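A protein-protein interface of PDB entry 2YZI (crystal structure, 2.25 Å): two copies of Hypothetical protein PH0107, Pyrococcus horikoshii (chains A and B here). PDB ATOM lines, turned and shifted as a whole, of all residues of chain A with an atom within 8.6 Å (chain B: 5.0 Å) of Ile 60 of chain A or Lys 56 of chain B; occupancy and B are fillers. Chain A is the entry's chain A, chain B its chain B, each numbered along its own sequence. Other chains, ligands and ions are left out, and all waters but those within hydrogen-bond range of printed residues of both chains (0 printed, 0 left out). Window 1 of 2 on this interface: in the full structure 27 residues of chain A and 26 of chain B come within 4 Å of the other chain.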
ATOM      1  N   VAL A  26      -3.708   8.121 -23.116  1.00  0.00           N
ATOM      2  CA  VAL A  26      -3.355   8.380 -21.731  1.00  0.00           C
ATOM      3  C   VAL A  26      -2.112   9.262 -21.702  1.00  0.00           C
ATOM      4  O   VAL A  26      -2.026  10.192 -20.906  1.00  0.00           O
ATOM      5  CB  VAL A  26      -3.083   7.057 -20.967  1.00  0.00           C
ATOM      6  CG1 VAL A  26      -2.500   7.346 -19.590  1.00  0.00           C
ATOM      7  CG2 VAL A  26      -4.383   6.281 -20.818  1.00  0.00           C
ATOM      8  N   SER A  30      -1.949  13.184 -20.434  1.00  0.00           N
ATOM      9  CA  SER A  30      -0.976  13.532 -19.417  1.00  0.00           C
ATOM     10  C   SER A  30      -0.126  14.719 -19.839  1.00  0.00           C
ATOM     11  O   SER A  30       0.174  15.596 -19.021  1.00  0.00           O
ATOM     12  CB  SER A  30      -0.099  12.327 -19.111  1.00  0.00           C
ATOM     13  OG  SER A  30      -0.864  11.310 -18.492  1.00  0.00           O
ATOM     14  N   MET A  33      -2.269  17.722 -19.556  1.00  0.00           N
ATOM     15  CA  MET A  33      -2.425  18.146 -18.169  1.00  0.00           C
ATOM     16  C   MET A  33      -1.221  18.946 -17.672  1.00  0.00           C
ATOM     17  O   MET A  33      -1.386  19.925 -16.949  1.00  0.00           O
ATOM     18  CB  MET A  33      -2.640  16.942 -17.248  1.00  0.00           C
ATOM     19  CG  MET A  33      -4.012  16.291 -17.348  1.00  0.00           C
ATOM     20  SD  MET A  33      -4.186  14.827 -16.063  1.00  0.00           S
ATOM     21  CE  MET A  33      -3.004  13.599 -16.919  1.00  0.00           C
ATOM     22  N   MET A  34      -0.016  18.527 -18.046  1.00  0.00           N
ATOM     23  CA  MET A  34       1.178  19.245 -17.614  1.00  0.00           C
ATOM     24  C   MET A  34       1.241  20.612 -18.287  1.00  0.00           C
ATOM     25  O   MET A  34       1.539  21.617 -17.641  1.00  0.00           O
ATOM     26  CB  MET A  34       2.451  18.443 -17.925  1.00  0.00           C
ATOM     27  CG  MET A  34       2.555  17.112 -17.169  1.00  0.00           C
ATOM     28  SD  MET A  34       2.257  17.283 -15.228  1.00  0.00           S
ATOM     29  CE  MET A  34       2.224  15.423 -14.755  1.00  0.00           C
ATOM     30  N   PHE A  54     -11.178  11.784 -15.180  1.00  0.00           N
ATOM     31  CA  PHE A  54     -10.029  11.095 -14.619  1.00  0.00           C
ATOM     32  C   PHE A  54      -8.983  12.097 -14.154  1.00  0.00           C
ATOM     33  O   PHE A  54      -8.776  13.142 -14.773  1.00  0.00           O
ATOM     34  CB  PHE A  54      -9.432  10.119 -15.643  1.00  0.00           C
ATOM     35  CG  PHE A  54      -8.914  10.777 -16.880  1.00  0.00           C
ATOM     36  CD1 PHE A  54      -7.628  11.294 -16.922  1.00  0.00           C
ATOM     37  CD2 PHE A  54      -9.726  10.917 -17.993  1.00  0.00           C
ATOM     38  CE1 PHE A  54      -7.160  11.942 -18.062  1.00  0.00           C
ATOM     39  CE2 PHE A  54      -9.265  11.566 -19.140  1.00  0.00           C
ATOM     40  CZ  PHE A  54      -7.989  12.078 -19.176  1.00  0.00           C
ATOM     41  N   THR A  55      -8.334  11.770 -13.048  1.00  0.00           N
ATOM     42  CA  THR A  55      -7.308  12.624 -12.472  1.00  0.00           C
ATOM     43  C   THR A  55      -5.938  11.983 -12.663  1.00  0.00           C
ATOM     44  O   THR A  55      -5.829  10.832 -13.076  1.00  0.00           O
ATOM     45  CB  THR A  55      -7.511  12.781 -10.977  1.00  0.00           C
ATOM     46  OG1 THR A  55      -7.282  11.515 -10.351  1.00  0.00           O
ATOM     47  CG2 THR A  55      -8.926  13.234 -10.669  1.00  0.00           C
ATOM     48  N   LYS A  56      -4.896  12.739 -12.349  1.00  0.00           N
ATOM     49  CA  LYS A  56      -3.543  12.239 -12.458  1.00  0.00           C
ATOM     50  C   LYS A  56      -3.474  10.986 -11.607  1.00  0.00           C
ATOM     51  O   LYS A  56      -2.879   9.973 -12.001  1.00  0.00           O
ATOM     52  CB  LYS A  56      -2.557  13.271 -11.931  1.00  0.00           C
ATOM     53  CG  LYS A  56      -2.402  14.504 -12.801  1.00  0.00           C
ATOM     54  CD  LYS A  56      -1.325  15.408 -12.229  1.00  0.00           C
ATOM     55  CE  LYS A  56      -1.030  16.601 -13.123  1.00  0.00           C
ATOM     56  NZ  LYS A  56      -0.273  17.638 -12.360  1.00  0.00           N
ATOM     57  N   SER A  57      -4.106  11.061 -10.441  1.00  0.00           N
ATOM     58  CA  SER A  57      -4.132   9.945  -9.517  1.00  0.00           C
ATOM     59  C   SER A  57      -4.728   8.707 -10.194  1.00  0.00           C
ATOM     60  O   SER A  57      -4.171   7.619 -10.089  1.00  0.00           O
ATOM     61  CB  SER A  57      -4.938  10.323  -8.265  1.00  0.00           C
ATOM     62  OG  SER A  57      -4.934   9.288  -7.302  1.00  0.00           O
ATOM     63  N   ASP A  58      -5.845   8.872 -10.905  1.00  0.00           N
ATOM     64  CA  ASP A  58      -6.472   7.739 -11.584  1.00  0.00           C
ATOM     65  C   ASP A  58      -5.562   7.101 -12.634  1.00  0.00           C
ATOM     66  O   ASP A  58      -5.571   5.886 -12.812  1.00  0.00           O
ATOM     67  CB  ASP A  58      -7.792   8.156 -12.249  1.00  0.00           C
ATOM     68  CG  ASP A  58      -8.830   8.614 -11.249  1.00  0.00           C
ATOM     69  OD1 ASP A  58      -8.926   7.994 -10.179  1.00  0.00           O
ATOM     70  OD2 ASP A  58      -9.559   9.588 -11.529  1.00  0.00           O
ATOM     71  N   ILE A  59      -4.781   7.917 -13.336  1.00  0.00           N
ATOM     72  CA  ILE A  59      -3.880   7.402 -14.357  1.00  0.00           C
ATOM     73  C   ILE A  59      -2.910   6.426 -13.731  1.00  0.00           C
ATOM     74  O   ILE A  59      -2.637   5.363 -14.277  1.00  0.00           O
ATOM     75  CB  ILE A  59      -3.078   8.533 -15.029  1.00  0.00           C
ATOM     76  CG1 ILE A  59      -4.011   9.360 -15.912  1.00  0.00           C
ATOM     77  CG2 ILE A  59      -1.908   7.955 -15.817  1.00  0.00           C
ATOM     78  CD1 ILE A  59      -3.319  10.419 -16.704  1.00  0.00           C
ATOM     79  N   ILE A  60      -2.393   6.804 -12.573  1.00  0.00           N
ATOM     80  CA  ILE A  60      -1.447   5.976 -11.842  1.00  0.00           C
ATOM     81  C   ILE A  60      -2.086   4.668 -11.404  1.00  0.00           C
ATOM     82  O   ILE A  60      -1.526   3.590 -11.602  1.00  0.00           O
ATOM     83  CB  ILE A  60      -0.958   6.716 -10.595  1.00  0.00           C
ATOM     84  CG1 ILE A  60      -0.204   7.974 -11.011  1.00  0.00           C
ATOM     85  CG2 ILE A  60      -0.090   5.804  -9.754  1.00  0.00           C
ATOM     86  CD1 ILE A  60       0.024   8.923  -9.889  1.00  0.00           C
ATOM     87  N   ARG A  61      -3.264   4.782 -10.805  1.00  0.00           N
ATOM     88  CA  ARG A  61      -4.011   3.639 -10.298  1.00  0.00           C
ATOM     89  C   ARG A  61      -4.505   2.640 -11.350  1.00  0.00           C
ATOM     90  O   ARG A  61      -4.660   1.459 -11.048  1.00  0.00           O
ATOM     91  CB  ARG A  61      -5.199   4.141  -9.473  1.00  0.00           C
ATOM     92  CG  ARG A  61      -6.047   3.044  -8.860  1.00  0.00           C
ATOM     93  CD  ARG A  61      -6.970   3.595  -7.786  1.00  0.00           C
ATOM     94  NE  ARG A  61      -7.869   4.627  -8.300  1.00  0.00           N
ATOM     95  CZ  ARG A  61      -8.788   4.425  -9.238  1.00  0.00           C
ATOM     96  NH1 ARG A  61      -8.938   3.223  -9.776  1.00  0.00           N
ATOM     97  NH2 ARG A  61      -9.564   5.424  -9.635  1.00  0.00           N
ATOM     98  N   ARG A  62      -4.732   3.101 -12.580  1.00  0.00           N
ATOM     99  CA  ARG A  62      -5.235   2.226 -13.637  1.00  0.00           C
ATOM    100  C   ARG A  62      -4.292   1.981 -14.806  1.00  0.00           C
ATOM    101  O   ARG A  62      -4.622   1.230 -15.715  1.00  0.00           O
ATOM    102  CB  ARG A  62      -6.560   2.771 -14.174  1.00  0.00           C
ATOM    103  CG  ARG A  62      -7.670   2.788 -13.152  1.00  0.00           C
ATOM    104  CD  ARG A  62      -8.765   3.758 -13.553  1.00  0.00           C
ATOM    105  NE  ARG A  62      -9.817   3.817 -12.545  1.00  0.00           N
ATOM    106  CZ  ARG A  62     -10.827   4.681 -12.553  1.00  0.00           C
ATOM    107  NH1 ARG A  62     -10.938   5.583 -13.523  1.00  0.00           N
ATOM    108  NH2 ARG A  62     -11.736   4.636 -11.588  1.00  0.00           N
ATOM    109  N   VAL A  63      -3.124   2.608 -14.791  1.00  0.00           N
ATOM    110  CA  VAL A  63      -2.160   2.430 -15.871  1.00  0.00           C
ATOM    111  C   VAL A  63      -0.799   2.010 -15.329  1.00  0.00           C
ATOM    112  O   VAL A  63      -0.256   0.976 -15.720  1.00  0.00           O
ATOM    113  CB  VAL A  63      -2.008   3.735 -16.692  1.00  0.00           C
ATOM    114  CG1 VAL A  63      -0.985   3.551 -17.807  1.00  0.00           C
ATOM    115  CG2 VAL A  63      -3.350   4.129 -17.280  1.00  0.00           C
ATOM    116  N   ILE A  64      -0.255   2.809 -14.419  1.00  0.00           N
ATOM    117  CA  ILE A  64       1.045   2.531 -13.827  1.00  0.00           C
ATOM    118  C   ILE A  64       1.123   1.190 -13.086  1.00  0.00           C
ATOM    119  O   ILE A  64       1.955   0.342 -13.415  1.00  0.00           O
ATOM    120  CB  ILE A  64       1.451   3.654 -12.844  1.00  0.00           C
ATOM    121  CG1 ILE A  64       1.599   4.988 -13.591  1.00  0.00           C
ATOM    122  CG2 ILE A  64       2.751   3.279 -12.138  1.00  0.00           C
ATOM    123  CD1 ILE A  64       2.842   5.093 -14.446  1.00  0.00           C
ATOM    124  N   VAL A  65       0.265   1.000 -12.087  1.00  0.00           N
ATOM    125  CA  VAL A  65       0.285  -0.230 -11.299  1.00  0.00           C
ATOM    126  C   VAL A  65      -0.111  -1.519 -12.015  1.00  0.00           C
ATOM    127  O   VAL A  65       0.362  -2.592 -11.654  1.00  0.00           O
ATOM    128  CB  VAL A  65      -0.582  -0.102 -10.016  1.00  0.00           C
ATOM    129  CG1 VAL A  65       0.076   0.842  -9.031  1.00  0.00           C
ATOM    130  CG2 VAL A  65      -1.956   0.395 -10.363  1.00  0.00           C
ATOM    131  N   PRO A  66      -0.992  -1.441 -13.026  1.00  0.00           N
ATOM    132  CA  PRO A  66      -1.384  -2.668 -13.723  1.00  0.00           C
ATOM    133  C   PRO A  66      -0.439  -3.022 -14.866  1.00  0.00           C
ATOM    134  O   PRO A  66      -0.411  -4.162 -15.328  1.00  0.00           O
ATOM    135  CB  PRO A  66      -2.788  -2.342 -14.206  1.00  0.00           C
ATOM    136  CG  PRO A  66      -2.662  -0.908 -14.567  1.00  0.00           C
ATOM    137  CD  PRO A  66      -1.864  -0.320 -13.423  1.00  0.00           C
ATOM    138  N   GLY A  67       0.323  -2.039 -15.328  1.00  0.00           N
ATOM    139  CA  GLY A  67       1.268  -2.284 -16.403  1.00  0.00           C
ATOM    140  C   GLY A  67       0.832  -1.852 -17.789  1.00  0.00           C
ATOM    141  O   GLY A  67       1.662  -1.758 -18.692  1.00  0.00           O
ATOM    142  N   LEU A  68      -0.461  -1.592 -17.960  1.00  0.00           N
ATOM    143  CA  LEU A  68      -1.001  -1.172 -19.252  1.00  0.00           C
ATOM    144  C   LEU A  68      -0.109  -0.147 -19.939  1.00  0.00           C
ATOM    145  O   LEU A  68       0.568   0.638 -19.281  1.00  0.00           O
ATOM    146  CB  LEU A  68      -2.404  -0.581 -19.080  1.00  0.00           C
ATOM    147  CG  LEU A  68      -3.577  -1.530 -18.794  1.00  0.00           C
ATOM    148  CD1 LEU A  68      -3.687  -2.552 -19.915  1.00  0.00           C
ATOM    149  CD2 LEU A  68      -3.386  -2.224 -17.465  1.00  0.00           C
ATOM    150  N   ILE A  77      -9.774   4.210 -19.028  1.00  0.00           N
ATOM    151  CA  ILE A  77      -9.408   4.463 -17.637  1.00  0.00           C
ATOM    152  C   ILE A  77     -10.254   5.545 -16.971  1.00  0.00           C
ATOM    153  O   ILE A  77     -10.024   5.899 -15.821  1.00  0.00           O
ATOM    154  CB  ILE A  77      -7.936   4.891 -17.530  1.00  0.00           C
ATOM    155  CG1 ILE A  77      -7.750   6.267 -18.173  1.00  0.00           C
ATOM    156  CG2 ILE A  77      -7.047   3.862 -18.219  1.00  0.00           C
ATOM    157  CD1 ILE A  77      -6.360   6.837 -18.010  1.00  0.00           C
ATOM    158  N   LYS A 104     -10.798  14.033  -4.118  1.00  0.00           N
ATOM    159  CA  LYS A 104     -10.129  15.324  -3.968  1.00  0.00           C
ATOM    160  C   LYS A 104     -10.498  16.253  -5.119  1.00  0.00           C
ATOM    161  O   LYS A 104      -9.871  17.290  -5.321  1.00  0.00           O
ATOM    162  CB  LYS A 104      -8.611  15.127  -3.936  1.00  0.00           C
ATOM    163  CG  LYS A 104      -8.148  13.997  -3.018  1.00  0.00           C
ATOM    164  CD  LYS A 104      -6.665  14.095  -2.700  1.00  0.00           C
ATOM    165  CE  LYS A 104      -6.121  12.765  -2.226  1.00  0.00           C
ATOM    166  NZ  LYS A 104      -7.018  12.127  -1.222  1.00  0.00           N
ATOM    167  N   SER B  30       4.015   3.495  -6.744  1.00  0.00           N
ATOM    168  CA  SER B  30       2.644   3.847  -7.108  1.00  0.00           C
ATOM    169  C   SER B  30       1.624   3.007  -6.342  1.00  0.00           C
ATOM    170  O   SER B  30       0.615   3.525  -5.869  1.00  0.00           O
ATOM    171  CB  SER B  30       2.411   3.667  -8.613  1.00  0.00           C
ATOM    172  OG  SER B  30       3.048   4.685  -9.363  1.00  0.00           O
ATOM    173  N   MET B  33       1.455   4.000  -2.711  1.00  0.00           N
ATOM    174  CA  MET B  33       0.739   5.265  -2.564  1.00  0.00           C
ATOM    175  C   MET B  33      -0.770   5.063  -2.596  1.00  0.00           C
ATOM    176  O   MET B  33      -1.508   5.693  -1.840  1.00  0.00           O
ATOM    177  CB  MET B  33       1.133   6.239  -3.679  1.00  0.00           C
ATOM    178  CG  MET B  33       2.531   6.818  -3.567  1.00  0.00           C
ATOM    179  SD  MET B  33       2.988   7.705  -5.243  1.00  0.00           S
ATOM    180  CE  MET B  33       2.915   9.563  -4.661  1.00  0.00           C
ATOM    181  N   MET B  34      -1.230   4.193  -3.485  1.00  0.00           N
ATOM    182  CA  MET B  34      -2.658   3.932  -3.593  1.00  0.00           C
ATOM    183  C   MET B  34      -3.133   3.144  -2.377  1.00  0.00           C
ATOM    184  O   MET B  34      -4.256   3.326  -1.923  1.00  0.00           O
ATOM    185  CB  MET B  34      -2.967   3.156  -4.879  1.00  0.00           C
ATOM    186  CG  MET B  34      -2.561   3.884  -6.155  1.00  0.00           C
ATOM    187  SD  MET B  34      -3.412   5.627  -6.302  1.00  0.00           S
ATOM    188  CE  MET B  34      -2.867   6.142  -8.075  1.00  0.00           C
ATOM    189  N   VAL B  38      -1.732   8.223  -0.043  1.00  0.00           N
ATOM    190  CA  VAL B  38      -0.897   9.420   0.036  1.00  0.00           C
ATOM    191  C   VAL B  38      -0.479   9.880  -1.356  1.00  0.00           C
ATOM    192  O   VAL B  38      -0.284   9.063  -2.260  1.00  0.00           O
ATOM    193  CB  VAL B  38       0.354   9.188   0.908  1.00  0.00           C
ATOM    194  CG1 VAL B  38      -0.066   8.947   2.347  1.00  0.00           C
ATOM    195  CG2 VAL B  38       1.160   8.019   0.378  1.00  0.00           C
ATOM    196  N   GLY B  39      -0.358  11.195  -1.529  1.00  0.00           N
ATOM    197  CA  GLY B  39       0.010  11.736  -2.823  1.00  0.00           C
ATOM    198  C   GLY B  39       1.500  11.905  -3.047  1.00  0.00           C
ATOM    199  O   GLY B  39       1.932  12.277  -4.139  1.00  0.00           O
ATOM    200  N   PHE B  54       9.031  12.970  -3.950  1.00  0.00           N
ATOM    201  CA  PHE B  54       8.297  12.999  -5.210  1.00  0.00           C
ATOM    202  C   PHE B  54       6.793  12.776  -5.030  1.00  0.00           C
ATOM    203  O   PHE B  54       6.339  12.131  -4.081  1.00  0.00           O
ATOM    204  CB  PHE B  54       8.889  11.983  -6.202  1.00  0.00           C
ATOM    205  CG  PHE B  54       8.600  10.547  -5.861  1.00  0.00           C
ATOM    206  CD1 PHE B  54       7.383   9.966  -6.212  1.00  0.00           C
ATOM    207  CD2 PHE B  54       9.560   9.766  -5.209  1.00  0.00           C
ATOM    208  CE1 PHE B  54       7.126   8.623  -5.923  1.00  0.00           C
ATOM    209  CE2 PHE B  54       9.315   8.421  -4.915  1.00  0.00           C
ATOM    210  CZ  PHE B  54       8.098   7.846  -5.271  1.00  0.00           C
ATOM    211  N   THR B  55       6.026  13.331  -5.960  1.00  0.00           N
ATOM    212  CA  THR B  55       4.571  13.238  -5.922  1.00  0.00           C
ATOM    213  C   THR B  55       4.033  12.384  -7.052  1.00  0.00           C
ATOM    214  O   THR B  55       4.788  11.855  -7.859  1.00  0.00           O
ATOM    215  CB  THR B  55       3.929  14.624  -6.051  1.00  0.00           C
ATOM    216  OG1 THR B  55       4.202  15.148  -7.356  1.00  0.00           O
ATOM    217  CG2 THR B  55       4.480  15.569  -4.998  1.00  0.00           C
ATOM    218  N   LYS B  56       2.713  12.249  -7.087  1.00  0.00           N
ATOM    219  CA  LYS B  56       2.045  11.487  -8.128  1.00  0.00           C
ATOM    220  C   LYS B  56       2.198  12.292  -9.413  1.00  0.00           C
ATOM    221  O   LYS B  56       2.368  11.741 -10.503  1.00  0.00           O
ATOM    222  CB  LYS B  56       0.564  11.311  -7.781  1.00  0.00           C
ATOM    223  CG  LYS B  56       0.292  10.330  -6.642  1.00  0.00           C
ATOM    224  CD  LYS B  56      -1.202  10.219  -6.340  1.00  0.00           C
ATOM    225  CE  LYS B  56      -1.488   9.192  -5.241  1.00  0.00           C
ATOM    226  NZ  LYS B  56      -2.940   9.092  -4.879  1.00  0.00           N
ATOM    227  N   SER B  57       2.158  13.608  -9.260  1.00  0.00           N
ATOM    228  CA  SER B  57       2.297  14.502 -10.387  1.00  0.00           C
ATOM    229  C   SER B  57       3.658  14.308 -11.048  1.00  0.00           C
ATOM    230  O   SER B  57       3.751  14.312 -12.277  1.00  0.00           O
ATOM    231  CB  SER B  57       2.132  15.949  -9.930  1.00  0.00           C
ATOM    232  OG  SER B  57       1.997  16.809 -11.040  1.00  0.00           O
ATOM    233  N   ASP B  58       4.708  14.143 -10.244  1.00  0.00           N
ATOM    234  CA  ASP B  58       6.050  13.944 -10.790  1.00  0.00           C
ATOM    235  C   ASP B  58       6.042  12.685 -11.638  1.00  0.00           C
ATOM    236  O   ASP B  58       6.671  12.633 -12.692  1.00  0.00           O
ATOM    237  CB  ASP B  58       7.096  13.777  -9.682  1.00  0.00           C
ATOM    238  CG  ASP B  58       7.215  14.993  -8.798  1.00  0.00           C
ATOM    239  OD1 ASP B  58       7.218  16.131  -9.318  1.00  0.00           O
ATOM    240  OD2 ASP B  58       7.322  14.810  -7.573  1.00  0.00           O
ATOM    241  N   ILE B  59       5.333  11.670 -11.155  1.00  0.00           N
ATOM    242  CA  ILE B  59       5.221  10.399 -11.858  1.00  0.00           C
ATOM    243  C   ILE B  59       4.550  10.574 -13.218  1.00  0.00           C
ATOM    244  O   ILE B  59       4.946   9.935 -14.187  1.00  0.00           O
ATOM    245  CB  ILE B  59       4.434   9.379 -11.009  1.00  0.00           C
ATOM    246  CG1 ILE B  59       5.293   8.950  -9.820  1.00  0.00           C
ATOM    247  CG2 ILE B  59       4.028   8.178 -11.851  1.00  0.00           C
ATOM    248  CD1 ILE B  59       4.551   8.191  -8.755  1.00  0.00           C
ATOM    249  N   ILE B  60       3.550  11.450 -13.298  1.00  0.00           N
ATOM    250  CA  ILE B  60       2.863  11.675 -14.568  1.00  0.00           C
ATOM    251  C   ILE B  60       3.770  12.433 -15.543  1.00  0.00           C
ATOM    252  O   ILE B  60       3.930  12.034 -16.693  1.00  0.00           O
ATOM    253  CB  ILE B  60       1.543  12.480 -14.383  1.00  0.00           C
ATOM    254  CG1 ILE B  60       0.524  11.683 -13.563  1.00  0.00           C
ATOM    255  CG2 ILE B  60       0.933  12.794 -15.743  1.00  0.00           C
ATOM    256  CD1 ILE B  60      -0.033  10.473 -14.286  1.00  0.00           C
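Of the printed residues of chain B, Ser 57 of chain A touches Met 34 (2.8 Å) and Lys 56 (3.1 Å). Ile 60 of chain A touches just these residues of chain B: Ser 30, Met 34 and Lys 56. Val 63 of chain A touches none of the printed residues of chain B. Printed residues of chain B within 4 Å of Ile 64 of chain A: Ser 30. Of the printed residues of chain A, Met 34 of chain B touches Ser 57, Ile 60 and Arg 61. No residue of chain A comes within 4 Å of Thr 55 of chain B. Lys 56 of chain B touches just these residues of chain A: Ser 57 and Ile 60. The nearest residue of chain A that does not touch Lys 56 of chain B is Lys 56 of chain A (5.4 Å). The nearest printed residue of chain B that does not touch Val 65 of chain A is Met 34 of chain B (4.9 Å).
N of Ser 57 of chain A sits close to OG1 of Thr 55 of chain A. The backbone carbonyl oxygen of Val 26 of chain A lies within hydrogen-bond range of the side-chain hydroxyl of Ser 30 of chain A (2.9 Å). O of Ile 60 of chain A lies within hydrogen-bond range of N of Val 65 of chain A (3.2 Å). The side-chain amino group of Lys 56 of chain B lies within hydrogen-bond range of the side-chain sulfur of Met 34 of chain B (3.8 Å). The side-chain hydroxyl of Thr 55 of chain B sits close to the backbone NH of Ser 57 of chain B, at 3.2 Å. The backbone carbonyl oxygen of Ile 59 of chain A sits at hydrogen-bond distance from the backbone NH of Ile 64 of chain A.
NZ of Lys 56 of chain B lies within hydrogen-bond range of OG of Ser 57 of chain A, at 3.1 Å. NZ of Lys 56 of chain A sits at hydrogen-bond distance from OG of Ser 57 of chain B (2.8 Å).
Of the 12 printed residues of chain B, 5 touch a printed residue of chain A. Hydrophobic or aromatic side chains of chain B within 4 Å of the printed part of chain A: Met 34 and Ile 60. Printed residues of chain A that touch a printed residue of chain B: Ser 30, Met 34, Lys 56, Ser 57, Ile 59, Ile 60, Arg 61, Ile 64 and Val 65. Among the printed residues, 14 pairs touch across the chains.
Met 34 of chain A touches Ser 57 of chain B, and with the chains exchanged Ser 57 of chain A touches Met 34 of chain B. Met 34 of chain A touches Ile 60 of chain B, and with the chains exchanged Ile 60 of chain A touches Met 34 of chain B. Lys 56 of chain A touches Ile 60 of chain B, and with the chains exchanged Ile 60 of chain A touches Lys 56 of chain B. Ile 59 of chain A touches Ile 60 of chain B, but with the chains exchanged Ile 60 of chain A does not touch Ile 59 of chain B (4.3 Å). Of the 14 pairs that touch across the chains among the printed residues, 10 have their exchanged pair printed and touching as well.
Among the printed residues, merely in contact across the chains: Ser 57 of chain A with Met 34 of chain B (2.8 Å), Met 34 of chain A with Ile 60 of chain B (3.0 Å), Arg 61 of chain A with Met 34 of chain B (3.1 Å), Met 34 of chain A with Ser 57 of chain B (3.1 Å), Ile 64 of chain A with Ser 30 of chain B (3.1 Å), Ile 60 of chain A with Met 34 of chain B (3.2 Å), Ile 60 of chain A with Lys 56 of chain B (3.2 Å), Ile 60 of chain A with Ser 30 of chain B (3.4 Å), Ile 59 of chain A with Ile 60 of chain B (3.5 Å), Ser 30 of chain A with Ile 60 of chain B (3.6 Å), Lys 56 of chain A with Ile 60 of chain B (3.7 Å) and Val 65 of chain A with Ser 30 of chain B (3.7 Å).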
